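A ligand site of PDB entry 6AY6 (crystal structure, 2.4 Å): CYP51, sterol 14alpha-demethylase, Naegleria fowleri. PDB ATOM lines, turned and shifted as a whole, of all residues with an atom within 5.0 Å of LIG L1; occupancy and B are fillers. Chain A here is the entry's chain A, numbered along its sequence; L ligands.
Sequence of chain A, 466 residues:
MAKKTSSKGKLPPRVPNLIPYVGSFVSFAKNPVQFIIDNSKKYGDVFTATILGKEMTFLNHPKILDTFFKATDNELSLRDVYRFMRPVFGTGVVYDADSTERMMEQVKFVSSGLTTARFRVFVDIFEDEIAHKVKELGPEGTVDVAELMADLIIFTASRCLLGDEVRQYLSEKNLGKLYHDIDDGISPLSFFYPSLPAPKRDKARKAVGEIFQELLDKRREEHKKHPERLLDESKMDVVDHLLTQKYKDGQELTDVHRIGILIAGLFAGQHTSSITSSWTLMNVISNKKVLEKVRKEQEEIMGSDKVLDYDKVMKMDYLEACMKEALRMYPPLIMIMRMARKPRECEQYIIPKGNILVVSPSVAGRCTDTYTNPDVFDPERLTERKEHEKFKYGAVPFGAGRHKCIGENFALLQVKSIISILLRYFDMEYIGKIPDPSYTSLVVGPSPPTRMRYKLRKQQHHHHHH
The side-chain sulfur (SG) of Cys 405 binds an iron atom (FE1) of LIG L1 (2.1 Å).
A ring nitrogen (ND1) of His 403 is in hydrogen-bond range of an oxygen (O4) of LIG L1, 2.8 Å away.
An oxygen (O2) of LIG L1 lies within salt-bridge range of the guanidinium group of Arg 338, at 2.8 Å.
The side-chain hydroxyl (OH) of Tyr 82 lies within hydrogen-bond range of an oxygen (O1) of LIG L1.
The side-chain hydroxyl of Tyr 95 is in hydrogen-bond range of an oxygen (O3) of LIG L1 (3.2 Å).
A nitrogen (N4) of LG2 L2 binds an iron atom (FE1) of LIG L1 (1.8 Å).
The backbone NH of Cys 405 is in hydrogen-bond range of the backbone carbonyl oxygen of Phe 398, 2.7 Å away.
The backbone NH (N) of Gly 407 sits close to the side-chain sulfur (SG) of Cys 405 (3.1 Å).
OH of Tyr 82 lies within hydrogen-bond range of N of Met 337 (3.1 Å).
The side-chain hydroxyl of Thr 272 is in hydrogen-bond range of the backbone carbonyl oxygen of Ala 268.
O of Thr 272 lies within hydrogen-bond range of OG1 of Thr 276, at 2.6 Å.
NZ of Lys 404 is in salt-bridge range of OE1 of Glu 408 (3.0 Å).
Gly 265 touches LIG L1.
Ala 268 touches LIG L1 (CB to C4, 3.5 Å).
Gly 269 touches LIG L1.
Thr 272 touches LIG L1 (OG1 to C15, 3.2 Å).
Ser 273 touches LIG L1.
CG of Pro 332 touches C17 of LIG L1 (3.98 Å).
CD1 of Leu 333 touches C2 of LIG L1 (3.4 Å).
Ile 336 touches LIG L1.
Pro 397 touches LIG L1.
Phe 398 touches LIG L1 (CE1 to C15, 3.3 Å).
Gly 399 touches LIG L1.
Arg 402 touches LIG L1.
Lys 404 touches LIG L1.
CG1 of Ile 406 touches C31 of LIG L1 (3.4 Å).
Gly 407 touches LIG L1 (CA to C22, 3.4 Å).
CD2 of Phe 410 touches C24 of LIG L1 (3.9 Å).
CB of Ala 411 touches C19 of LIG L1 (3.4 Å).
Hydrophobic or aromatic side chains that line LIG L1: Tyr 82, Ala 268, Pro 332, Leu 333, Ile 336, Phe 398, His 403, Ile 406, Phe 410 and Ala 411.
Of the 32 residues printed, 22 come within 4 Å of LIG L1.
The nearest printed residue that does not touch LIG L1 is Leu 327 (4.1 Å).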
ATOM      1  N   LEU A  78      -1.219  -9.811  26.941  1.00  0.00           N
ATOM      2  CA  LEU A  78      -1.284  -8.760  27.934  1.00  0.00           C
ATOM      3  C   LEU A  78      -2.518  -8.923  28.719  1.00  0.00           C
ATOM      4  O   LEU A  78      -2.510  -8.876  29.944  1.00  0.00           O
ATOM      5  CB  LEU A  78      -1.325  -7.397  27.279  1.00  0.00           C
ATOM      6  CG  LEU A  78       0.024  -6.881  26.903  1.00  0.00           C
ATOM      7  CD1 LEU A  78       0.431  -7.538  25.594  1.00  0.00           C
ATOM      8  CD2 LEU A  78      -0.018  -5.381  26.793  1.00  0.00           C
ATOM      9  N   TYR A  82      -2.836  -8.101  32.905  1.00  0.00           N
ATOM     10  CA  TYR A  82      -3.226  -6.760  33.411  1.00  0.00           C
ATOM     11  C   TYR A  82      -4.736  -6.602  33.495  1.00  0.00           C
ATOM     12  O   TYR A  82      -5.258  -5.496  33.448  1.00  0.00           O
ATOM     13  CB  TYR A  82      -2.684  -5.649  32.516  1.00  0.00           C
ATOM     14  CG  TYR A  82      -1.205  -5.705  32.252  1.00  0.00           C
ATOM     15  CD1 TYR A  82      -0.293  -5.725  33.289  1.00  0.00           C
ATOM     16  CD2 TYR A  82      -0.713  -5.607  30.947  1.00  0.00           C
ATOM     17  CE1 TYR A  82       1.066  -5.697  33.048  1.00  0.00           C
ATOM     18  CE2 TYR A  82       0.641  -5.599  30.694  1.00  0.00           C
ATOM     19  CZ  TYR A  82       1.527  -5.640  31.744  1.00  0.00           C
ATOM     20  OH  TYR A  82       2.881  -5.590  31.493  1.00  0.00           O
ATOM     21  N   TYR A  95      -7.551  -3.694  28.576  1.00  0.00           N
ATOM     22  CA  TYR A  95      -6.955  -5.023  28.819  1.00  0.00           C
ATOM     23  C   TYR A  95      -8.016  -6.015  29.281  1.00  0.00           C
ATOM     24  O   TYR A  95      -7.789  -7.242  29.266  1.00  0.00           O
ATOM     25  CB  TYR A  95      -5.839  -4.939  29.842  1.00  0.00           C
ATOM     26  CG  TYR A  95      -4.638  -4.195  29.353  1.00  0.00           C
ATOM     27  CD1 TYR A  95      -3.958  -4.609  28.199  1.00  0.00           C
ATOM     28  CD2 TYR A  95      -4.203  -3.042  29.985  1.00  0.00           C
ATOM     29  CE1 TYR A  95      -2.870  -3.900  27.721  1.00  0.00           C
ATOM     30  CE2 TYR A  95      -3.111  -2.327  29.518  1.00  0.00           C
ATOM     31  CZ  TYR A  95      -2.450  -2.755  28.380  1.00  0.00           C
ATOM     32  OH  TYR A  95      -1.365  -2.032  27.912  1.00  0.00           O
ATOM     33  N   VAL A 107      -6.965   2.228  22.762  1.00  0.00           N
ATOM     34  CA  VAL A 107      -5.663   2.859  22.823  1.00  0.00           C
ATOM     35  C   VAL A 107      -5.508   4.002  21.818  1.00  0.00           C
ATOM     36  O   VAL A 107      -5.069   5.105  22.179  1.00  0.00           O
ATOM     37  CB  VAL A 107      -4.561   1.807  22.591  1.00  0.00           C
ATOM     38  CG1 VAL A 107      -3.203   2.481  22.472  1.00  0.00           C
ATOM     39  CG2 VAL A 107      -4.569   0.783  23.713  1.00  0.00           C
ATOM     40  N   VAL A 110      -7.074   7.460  22.501  1.00  0.00           N
ATOM     41  CA  VAL A 110      -6.177   8.243  23.341  1.00  0.00           C
ATOM     42  C   VAL A 110      -5.089   8.920  22.499  1.00  0.00           C
ATOM     43  O   VAL A 110      -4.981  10.145  22.458  1.00  0.00           O
ATOM     44  CB  VAL A 110      -5.499   7.347  24.402  1.00  0.00           C
ATOM     45  CG1 VAL A 110      -4.587   8.169  25.300  1.00  0.00           C
ATOM     46  CG2 VAL A 110      -6.545   6.621  25.222  1.00  0.00           C
ATOM     47  N   LEU A 114      -3.096  13.105  21.038  1.00  0.00           N
ATOM     48  CA  LEU A 114      -1.682  13.367  21.360  1.00  0.00           C
ATOM     49  C   LEU A 114      -0.917  13.757  20.099  1.00  0.00           C
ATOM     50  O   LEU A 114       0.125  13.157  19.778  1.00  0.00           O
ATOM     51  CB  LEU A 114      -1.032  12.133  21.963  1.00  0.00           C
ATOM     52  CG  LEU A 114      -1.575  11.546  23.274  1.00  0.00           C
ATOM     53  CD1 LEU A 114      -0.614  10.483  23.771  1.00  0.00           C
ATOM     54  CD2 LEU A 114      -1.802  12.624  24.329  1.00  0.00           C
ATOM     55  N   LEU A 161      -5.705  16.075  28.173  1.00  0.00           N
ATOM     56  CA  LEU A 161      -6.436  14.959  27.589  1.00  0.00           C
ATOM     57  C   LEU A 161      -7.959  15.185  27.590  1.00  0.00           C
ATOM     58  O   LEU A 161      -8.674  14.699  26.697  1.00  0.00           O
ATOM     59  CB  LEU A 161      -6.110  13.678  28.363  1.00  0.00           C
ATOM     60  CG  LEU A 161      -4.626  13.370  28.472  1.00  0.00           C
ATOM     61  CD1 LEU A 161      -4.421  11.999  29.086  1.00  0.00           C
ATOM     62  CD2 LEU A 161      -3.936  13.447  27.105  1.00  0.00           C
ATOM     63  N   GLY A 265      -6.322   6.320  30.381  1.00  0.00           N
ATOM     64  CA  GLY A 265      -5.333   7.259  29.856  1.00  0.00           C
ATOM     65  C   GLY A 265      -4.726   8.199  30.896  1.00  0.00           C
ATOM     66  O   GLY A 265      -3.526   8.504  30.843  1.00  0.00           O
ATOM     67  N   ALA A 268      -2.076   5.981  33.143  1.00  0.00           N
ATOM     68  CA  ALA A 268      -0.948   6.110  32.204  1.00  0.00           C
ATOM     69  C   ALA A 268      -0.368   7.510  32.223  1.00  0.00           C
ATOM     70  O   ALA A 268       0.835   7.700  32.342  1.00  0.00           O
ATOM     71  CB  ALA A 268      -1.408   5.773  30.805  1.00  0.00           C
ATOM     72  N   GLY A 269      -1.244   8.499  32.067  1.00  0.00           N
ATOM     73  CA  GLY A 269      -0.813   9.872  31.817  1.00  0.00           C
ATOM     74  C   GLY A 269      -0.066  10.550  32.966  1.00  0.00           C
ATOM     75  O   GLY A 269       0.624  11.535  32.747  1.00  0.00           O
ATOM     76  N   THR A 272       3.650   7.594  35.813  1.00  0.00           N
ATOM     77  CA  THR A 272       4.983   7.369  35.254  1.00  0.00           C
ATOM     78  C   THR A 272       5.679   8.696  34.989  1.00  0.00           C
ATOM     79  O   THR A 272       6.889   8.806  35.158  1.00  0.00           O
ATOM     80  CB  THR A 272       4.925   6.611  33.952  1.00  0.00           C
ATOM     81  OG1 THR A 272       4.080   7.325  33.036  1.00  0.00           O
ATOM     82  CG2 THR A 272       4.384   5.213  34.172  1.00  0.00           C
ATOM     83  N   SER A 273       4.910   9.664  34.509  1.00  0.00           N
ATOM     84  CA  SER A 273       5.433  10.983  34.178  1.00  0.00           C
ATOM     85  C   SER A 273       6.037  11.681  35.403  1.00  0.00           C
ATOM     86  O   SER A 273       7.134  12.249  35.345  1.00  0.00           O
ATOM     87  CB  SER A 273       4.320  11.847  33.601  1.00  0.00           C
ATOM     88  OG  SER A 273       4.223  11.696  32.203  1.00  0.00           O
ATOM     89  N   THR A 276       8.937  10.488  36.995  1.00  0.00           N
ATOM     90  CA  THR A 276      10.111  10.648  36.132  1.00  0.00           C
ATOM     91  C   THR A 276      10.659  12.080  36.247  1.00  0.00           C
ATOM     92  O   THR A 276      11.875  12.286  36.318  1.00  0.00           O
ATOM     93  CB  THR A 276       9.795  10.292  34.656  1.00  0.00           C
ATOM     94  OG1 THR A 276       9.449   8.900  34.554  1.00  0.00           O
ATOM     95  CG2 THR A 276      10.993  10.574  33.742  1.00  0.00           C
ATOM     96  N   LEU A 327      15.377   7.522  33.563  1.00  0.00           N
ATOM     97  CA  LEU A 327      14.629   6.327  33.146  1.00  0.00           C
ATOM     98  C   LEU A 327      15.498   5.051  33.081  1.00  0.00           C
ATOM     99  O   LEU A 327      14.996   3.947  33.210  1.00  0.00           O
ATOM    100  CB  LEU A 327      13.953   6.557  31.788  1.00  0.00           C
ATOM    101  CG  LEU A 327      12.729   7.476  31.723  1.00  0.00           C
ATOM    102  CD1 LEU A 327      12.430   7.847  30.284  1.00  0.00           C
ATOM    103  CD2 LEU A 327      11.523   6.817  32.380  1.00  0.00           C
ATOM    104  N   PRO A 332       9.792   3.541  36.052  1.00  0.00           N
ATOM    105  CA  PRO A 332       8.700   3.396  37.021  1.00  0.00           C
ATOM    106  C   PRO A 332       7.875   2.093  36.828  1.00  0.00           C
ATOM    107  O   PRO A 332       7.155   1.676  37.747  1.00  0.00           O
ATOM    108  CB  PRO A 332       7.837   4.624  36.754  1.00  0.00           C
ATOM    109  CG  PRO A 332       8.129   5.000  35.347  1.00  0.00           C
ATOM    110  CD  PRO A 332       9.561   4.644  35.119  1.00  0.00           C
ATOM    111  N   LEU A 333       7.928   1.541  35.627  1.00  0.00           N
ATOM    112  CA  LEU A 333       7.444   0.214  35.388  1.00  0.00           C
ATOM    113  C   LEU A 333       8.645  -0.735  35.342  1.00  0.00           C
ATOM    114  O   LEU A 333       9.400  -0.754  34.360  1.00  0.00           O
ATOM    115  CB  LEU A 333       6.644   0.174  34.088  1.00  0.00           C
ATOM    116  CG  LEU A 333       5.550   1.260  34.044  1.00  0.00           C
ATOM    117  CD1 LEU A 333       4.919   1.391  32.673  1.00  0.00           C
ATOM    118  CD2 LEU A 333       4.491   0.997  35.099  1.00  0.00           C
ATOM    119  N   ILE A 336       7.711  -5.730  32.885  1.00  0.00           N
ATOM    120  CA  ILE A 336       6.778  -5.925  31.771  1.00  0.00           C
ATOM    121  C   ILE A 336       6.411  -7.383  31.713  1.00  0.00           C
ATOM    122  O   ILE A 336       7.297  -8.233  31.764  1.00  0.00           O
ATOM    123  CB  ILE A 336       7.433  -5.572  30.428  1.00  0.00           C
ATOM    124  CG1 ILE A 336       7.834  -4.103  30.382  1.00  0.00           C
ATOM    125  CG2 ILE A 336       6.498  -5.886  29.277  1.00  0.00           C
ATOM    126  CD1 ILE A 336       8.766  -3.784  29.234  1.00  0.00           C
ATOM    127  N   MET A 337       5.131  -7.689  31.517  1.00  0.00           N
ATOM    128  CA  MET A 337       4.657  -9.070  31.651  1.00  0.00           C
ATOM    129  C   MET A 337       3.676  -9.499  30.555  1.00  0.00           C
ATOM    130  O   MET A 337       2.829  -8.722  30.097  1.00  0.00           O
ATOM    131  CB  MET A 337       4.031  -9.291  33.039  1.00  0.00           C
ATOM    132  CG  MET A 337       5.007  -9.104  34.185  1.00  0.00           C
ATOM    133  SD  MET A 337       4.203  -9.142  35.793  1.00  0.00           S
ATOM    134  CE  MET A 337       3.357  -7.558  35.775  1.00  0.00           C
ATOM    135  N   ARG A 338       3.808 -10.756  30.151  1.00  0.00           N
ATOM    136  CA  ARG A 338       2.879 -11.393  29.225  1.00  0.00           C
ATOM    137  C   ARG A 338       2.585 -12.788  29.759  1.00  0.00           C
ATOM    138  O   ARG A 338       3.482 -13.434  30.287  1.00  0.00           O
ATOM    139  CB  ARG A 338       3.520 -11.512  27.857  1.00  0.00           C
ATOM    140  CG  ARG A 338       4.045 -10.197  27.299  1.00  0.00           C
ATOM    141  CD  ARG A 338       2.971  -9.439  26.562  1.00  0.00           C
ATOM    142  NE  ARG A 338       3.500  -8.273  25.864  1.00  0.00           N
ATOM    143  CZ  ARG A 338       3.726  -7.092  26.431  1.00  0.00           C
ATOM    144  NH1 ARG A 338       3.470  -6.918  27.728  1.00  0.00           N
ATOM    145  NH2 ARG A 338       4.197  -6.080  25.711  1.00  0.00           N
ATOM    146  N   VAL A 396      14.855   0.156  27.579  1.00  0.00           N
ATOM    147  CA  VAL A 396      13.441  -0.165  27.306  1.00  0.00           C
ATOM    148  C   VAL A 396      12.421   0.503  28.277  1.00  0.00           C
ATOM    149  O   VAL A 396      11.352  -0.054  28.530  1.00  0.00           O
ATOM    150  CB  VAL A 396      13.234  -1.693  27.328  1.00  0.00           C
ATOM    151  CG1 VAL A 396      13.633  -2.307  25.998  1.00  0.00           C
ATOM    152  CG2 VAL A 396      14.015  -2.325  28.469  1.00  0.00           C
ATOM    153  N   PRO A 397      12.678   1.753  28.701  1.00  0.00           N
ATOM    154  CA  PRO A 397      11.712   2.329  29.652  1.00  0.00           C
ATOM    155  C   PRO A 397      10.283   2.475  29.095  1.00  0.00           C
ATOM    156  O   PRO A 397       9.331   2.464  29.878  1.00  0.00           O
ATOM    157  CB  PRO A 397      12.306   3.702  29.953  1.00  0.00           C
ATOM    158  CG  PRO A 397      13.162   4.029  28.785  1.00  0.00           C
ATOM    159  CD  PRO A 397      13.722   2.714  28.305  1.00  0.00           C
ATOM    160  N   PHE A 398      10.128   2.618  27.777  1.00  0.00           N
ATOM    161  CA  PHE A 398       8.802   2.759  27.133  1.00  0.00           C
ATOM    162  C   PHE A 398       8.365   1.507  26.361  1.00  0.00           C
ATOM    163  O   PHE A 398       7.512   1.582  25.467  1.00  0.00           O
ATOM    164  CB  PHE A 398       8.805   3.938  26.182  1.00  0.00           C
ATOM    165  CG  PHE A 398       8.917   5.256  26.860  1.00  0.00           C
ATOM    166  CD1 PHE A 398       7.789   5.937  27.297  1.00  0.00           C
ATOM    167  CD2 PHE A 398      10.151   5.846  27.037  1.00  0.00           C
ATOM    168  CE1 PHE A 398       7.892   7.166  27.917  1.00  0.00           C
ATOM    169  CE2 PHE A 398      10.260   7.090  27.638  1.00  0.00           C
ATOM    170  CZ  PHE A 398       9.137   7.758  28.055  1.00  0.00           C
ATOM    171  N   GLY A 399       8.922   0.356  26.716  1.00  0.00           N
ATOM    172  CA  GLY A 399       8.616  -0.853  26.033  1.00  0.00           C
ATOM    173  C   GLY A 399       9.211  -0.837  24.659  1.00  0.00           C
ATOM    174  O   GLY A 399      10.108  -0.035  24.361  1.00  0.00           O
ATOM    175  N   ARG A 402       5.077  -4.375  19.611  1.00  0.00           N
ATOM    176  CA  ARG A 402       3.684  -4.198  19.251  1.00  0.00           C
ATOM    177  C   ARG A 402       2.953  -3.295  20.258  1.00  0.00           C
ATOM    178  O   ARG A 402       1.967  -2.655  19.902  1.00  0.00           O
ATOM    179  CB  ARG A 402       2.978  -5.556  19.129  1.00  0.00           C
ATOM    180  CG  ARG A 402       1.533  -5.455  18.627  1.00  0.00           C
ATOM    181  CD  ARG A 402       0.936  -6.820  18.316  1.00  0.00           C
ATOM    182  NE  ARG A 402       1.538  -7.422  17.133  1.00  0.00           N
ATOM    183  CZ  ARG A 402       2.609  -8.203  17.153  1.00  0.00           C
ATOM    184  NH1 ARG A 402       3.197  -8.500  18.310  1.00  0.00           N
ATOM    185  NH2 ARG A 402       3.089  -8.714  16.026  1.00  0.00           N
ATOM    186  N   HIS A 403       3.476  -3.197  21.477  1.00  0.00           N
ATOM    187  CA  HIS A 403       2.838  -2.368  22.515  1.00  0.00           C
ATOM    188  C   HIS A 403       3.732  -1.262  23.121  1.00  0.00           C
ATOM    189  O   HIS A 403       3.297  -0.549  24.011  1.00  0.00           O
ATOM    190  CB  HIS A 403       2.303  -3.264  23.628  1.00  0.00           C
ATOM    191  CG  HIS A 403       1.322  -4.283  23.168  1.00  0.00           C
ATOM    192  ND1 HIS A 403       0.007  -3.976  22.887  1.00  0.00           N
ATOM    193  CD2 HIS A 403       1.460  -5.603  22.898  1.00  0.00           C
ATOM    194  CE1 HIS A 403      -0.621  -5.058  22.466  1.00  0.00           C
ATOM    195  NE2 HIS A 403       0.251  -6.060  22.444  1.00  0.00           N
ATOM    196  N   LYS A 404       4.907  -1.017  22.542  1.00  0.00           N
ATOM    197  CA  LYS A 404       5.665   0.196  22.868  1.00  0.00           C
ATOM    198  C   LYS A 404       4.719   1.361  23.354  1.00  0.00           C
ATOM    199  O   LYS A 404       3.561   1.440  22.927  1.00  0.00           O
ATOM    200  CB  LYS A 404       6.467   0.627  21.639  1.00  0.00           C
ATOM    201  CG  LYS A 404       7.645   1.552  21.950  1.00  0.00           C
ATOM    202  CD  LYS A 404       8.375   1.992  20.692  1.00  0.00           C
ATOM    203  CE  LYS A 404       9.264   3.214  20.940  1.00  0.00           C
ATOM    204  NZ  LYS A 404       9.936   3.183  22.275  1.00  0.00           N
ATOM    205  N   CYS A 405       5.181   2.210  24.269  1.00  0.00           N
ATOM    206  CA  CYS A 405       4.286   3.235  24.855  1.00  0.00           C
ATOM    207  C   CYS A 405       3.834   4.219  23.806  1.00  0.00           C
ATOM    208  O   CYS A 405       4.632   4.856  23.145  1.00  0.00           O
ATOM    209  CB  CYS A 405       4.961   3.998  26.009  1.00  0.00           C
ATOM    210  SG  CYS A 405       3.797   5.142  26.850  1.00  0.00           S
ATOM    211  N   ILE A 406       2.523   4.378  23.664  1.00  0.00           N
ATOM    212  CA  ILE A 406       1.973   5.418  22.799  1.00  0.00           C
ATOM    213  C   ILE A 406       1.978   6.802  23.473  1.00  0.00           C
ATOM    214  O   ILE A 406       1.433   7.756  22.916  1.00  0.00           O
ATOM    215  CB  ILE A 406       0.515   5.105  22.359  1.00  0.00           C
ATOM    216  CG1 ILE A 406      -0.432   5.074  23.567  1.00  0.00           C
ATOM    217  CG2 ILE A 406       0.465   3.798  21.584  1.00  0.00           C
ATOM    218  CD1 ILE A 406      -1.317   6.291  23.688  1.00  0.00           C
ATOM    219  N   GLY A 407       2.576   6.892  24.659  1.00  0.00           N
ATOM    220  CA  GLY A 407       2.617   8.172  25.411  1.00  0.00           C
ATOM    221  C   GLY A 407       3.990   8.846  25.430  1.00  0.00           C
ATOM    222  O   GLY A 407       4.120  10.006  25.858  1.00  0.00           O
ATOM    223  N   GLU A 408       4.987   8.175  24.825  1.00  0.00           N
ATOM    224  CA  GLU A 408       6.397   8.555  24.924  1.00  0.00           C
ATOM    225  C   GLU A 408       6.623  10.037  24.656  1.00  0.00           C
ATOM    226  O   GLU A 408       7.320  10.700  25.408  1.00  0.00           O
ATOM    227  CB  GLU A 408       7.252   7.719  23.953  1.00  0.00           C
ATOM    228  CG  GLU A 408       8.673   8.263  23.721  1.00  0.00           C
ATOM    229  CD  GLU A 408       9.663   7.169  23.240  1.00  0.00           C
ATOM    230  OE1 GLU A 408       9.229   6.042  22.941  1.00  0.00           O
ATOM    231  OE2 GLU A 408      10.892   7.428  23.234  1.00  0.00           O
ATOM    232  N   PHE A 410       4.487  12.543  24.546  1.00  0.00           N
ATOM    233  CA  PHE A 410       3.778  13.472  25.446  1.00  0.00           C
ATOM    234  C   PHE A 410       4.471  13.462  26.788  1.00  0.00           C
ATOM    235  O   PHE A 410       4.642  14.491  27.407  1.00  0.00           O
ATOM    236  CB  PHE A 410       2.310  13.080  25.621  1.00  0.00           C
ATOM    237  CG  PHE A 410       1.582  13.896  26.666  1.00  0.00           C
ATOM    238  CD1 PHE A 410       1.316  15.248  26.449  1.00  0.00           C
ATOM    239  CD2 PHE A 410       1.107  13.301  27.828  1.00  0.00           C
ATOM    240  CE1 PHE A 410       0.600  15.985  27.380  1.00  0.00           C
ATOM    241  CE2 PHE A 410       0.399  14.045  28.762  1.00  0.00           C
ATOM    242  CZ  PHE A 410       0.162  15.383  28.541  1.00  0.00           C
ATOM    243  N   ALA A 411       4.970  12.304  27.168  1.00  0.00           N
ATOM    244  CA  ALA A 411       5.719  12.199  28.396  1.00  0.00           C
ATOM    245  C   ALA A 411       6.838  13.211  28.385  1.00  0.00           C
ATOM    246  O   ALA A 411       6.945  14.058  29.289  1.00  0.00           O
ATOM    247  CB  ALA A 411       6.275  10.803  28.563  1.00  0.00           C
HETATM  248  C1  LIG L   1       2.643   1.245  27.376  1.00  0.00           C
HETATM  249  C2  LIG L   1       6.150   3.140  29.970  1.00  0.00           C
HETATM  250  C3  LIG L   1       4.008   7.512  29.765  1.00  0.00           C
HETATM  251  C4  LIG L   1       0.226   5.375  27.719  1.00  0.00           C
HETATM  252  C5  LIG L   1       3.805   1.447  28.012  1.00  0.00           C
HETATM  253  C6  LIG L   1       4.785   0.454  28.217  1.00  0.00           C
HETATM  254  C7  LIG L   1       5.773   1.007  28.937  1.00  0.00           C
HETATM  255  C8  LIG L   1       5.393   2.301  29.236  1.00  0.00           C
HETATM  256  C9  LIG L   1       7.033   0.338  29.395  1.00  0.00           C
HETATM  257  C10 LIG L   1       4.784  -0.929  27.668  1.00  0.00           C
HETATM  258  C11 LIG L   1       3.796  -1.817  28.445  1.00  0.00           C
HETATM  259  C12 LIG L   1       3.991  -3.273  28.058  1.00  0.00           C
HETATM  260  O1  LIG L   1       3.563  -4.168  28.817  1.00  0.00           O
HETATM  261  O2  LIG L   1       4.593  -3.585  27.013  1.00  0.00           O
HETATM  262  C13 LIG L   1       5.852   4.482  30.127  1.00  0.00           C
HETATM  263  C14 LIG L   1       6.722   5.324  30.767  1.00  0.00           C
HETATM  264  C15 LIG L   1       6.204   6.564  30.747  1.00  0.00           C
HETATM  265  C16 LIG L   1       4.908   6.454  30.017  1.00  0.00           C
HETATM  266  C17 LIG L   1       8.046   4.952  31.369  1.00  0.00           C
HETATM  267  C18 LIG L   1       6.920   7.722  31.340  1.00  0.00           C
HETATM  268  C19 LIG L   1       6.384   8.931  31.387  1.00  0.00           C
HETATM  269  C20 LIG L   1       2.769   7.303  29.170  1.00  0.00           C
HETATM  270  C21 LIG L   1       1.815   8.278  28.889  1.00  0.00           C
HETATM  271  C22 LIG L   1       0.772   7.644  28.233  1.00  0.00           C
HETATM  272  C23 LIG L   1       1.076   6.289  28.191  1.00  0.00           C
HETATM  273  C24 LIG L   1       1.943   9.750  29.164  1.00  0.00           C
HETATM  274  C25 LIG L   1      -0.534   8.169  27.829  1.00  0.00           C
HETATM  275  C26 LIG L   1      -0.931   9.359  28.233  1.00  0.00           C
HETATM  276  C27 LIG L   1       0.614   4.086  27.474  1.00  0.00           C
HETATM  277  C28 LIG L   1      -0.255   3.176  26.770  1.00  0.00           C
HETATM  278  C29 LIG L   1       0.418   2.034  26.627  1.00  0.00           C
HETATM  279  C30 LIG L   1       1.703   2.246  27.297  1.00  0.00           C
HETATM  280  C31 LIG L   1      -1.665   3.443  26.316  1.00  0.00           C
HETATM  281  C32 LIG L   1      -0.133   0.758  26.063  1.00  0.00           C
HETATM  282  C33 LIG L   1       0.529   0.403  24.731  1.00  0.00           C
HETATM  283  C34 LIG L   1      -0.155  -0.812  24.124  1.00  0.00           C
HETATM  284  O3  LIG L   1      -1.041  -1.425  24.763  1.00  0.00           O
HETATM  285  O4  LIG L   1       0.151  -1.214  22.975  1.00  0.00           O
HETATM  286  N1  LIG L   1       4.187   2.562  28.701  1.00  0.00           N
HETATM  287  N2  LIG L   1       4.780   5.154  29.708  1.00  0.00           N
HETATM  288  N3  LIG L   1       2.252   6.104  28.763  1.00  0.00           N
HETATM  289  N4  LIG L   1       1.776   3.497  27.755  1.00  0.00           N
HETATM  290 FE1  LIG L   1       3.231   4.290  28.671  1.00  0.00          FE
HETATM  291  F1  LG2 L   2      -1.525   1.925  33.563  1.00  0.00           F
HETATM  292  F2  LG2 L   2       0.694  -0.357  36.055  1.00  0.00           F
HETATM  293  F3  LG2 L   2      -4.111   2.614  29.671  1.00  0.00           F
HETATM  294  O1  LG2 L   2       1.254  -0.159  31.212  1.00  0.00           O
HETATM  295  N1  LG2 L   2       1.643   2.752  31.806  1.00  0.00           N
HETATM  296  N2  LG2 L   2       1.965  -1.971  33.058  1.00  0.00           N
HETATM  297  N3  LG2 L   2       1.467   4.057  32.243  1.00  0.00           N
HETATM  298  N4  LG2 L   2       2.462   3.996  30.287  1.00  0.00           N
HETATM  299  N5  LG2 L   2       3.321  -2.518  34.913  1.00  0.00           N
HETATM  300  C1  LG2 L   2       0.460   0.535  32.162  1.00  0.00           C
HETATM  301  C2  LG2 L   2       0.041  -0.501  33.206  1.00  0.00           C
HETATM  302  C3  LG2 L   2       1.251   1.712  32.775  1.00  0.00           C
HETATM  303  C4  LG2 L   2      -0.759   1.059  31.480  1.00  0.00           C
HETATM  304  C5  LG2 L   2      -0.757  -1.598  32.543  1.00  0.00           C
HETATM  305  C6  LG2 L   2       1.203  -1.162  33.814  1.00  0.00           C
HETATM  306  C7  LG2 L   2      -1.751   1.771  32.265  1.00  0.00           C
HETATM  307  C8  LG2 L   2      -0.959   0.878  30.136  1.00  0.00           C
HETATM  308  C9  LG2 L   2       1.444  -1.129  35.266  1.00  0.00           C
HETATM  309  C10 LG2 L   2      -2.844   2.354  31.640  1.00  0.00           C
HETATM  310  C11 LG2 L   2      -2.107   1.389  29.545  1.00  0.00           C
HETATM  311  C12 LG2 L   2       2.325   2.719  30.681  1.00  0.00           C
HETATM  312  C13 LG2 L   2      -3.035   2.124  30.285  1.00  0.00           C
HETATM  313  C14 LG2 L   2       2.555  -1.805  35.757  1.00  0.00           C
HETATM  314  C15 LG2 L   2       3.021  -2.606  33.598  1.00  0.00           C
HETATM  315  C16 LG2 L   2       1.940   4.821  31.242  1.00  0.00           C
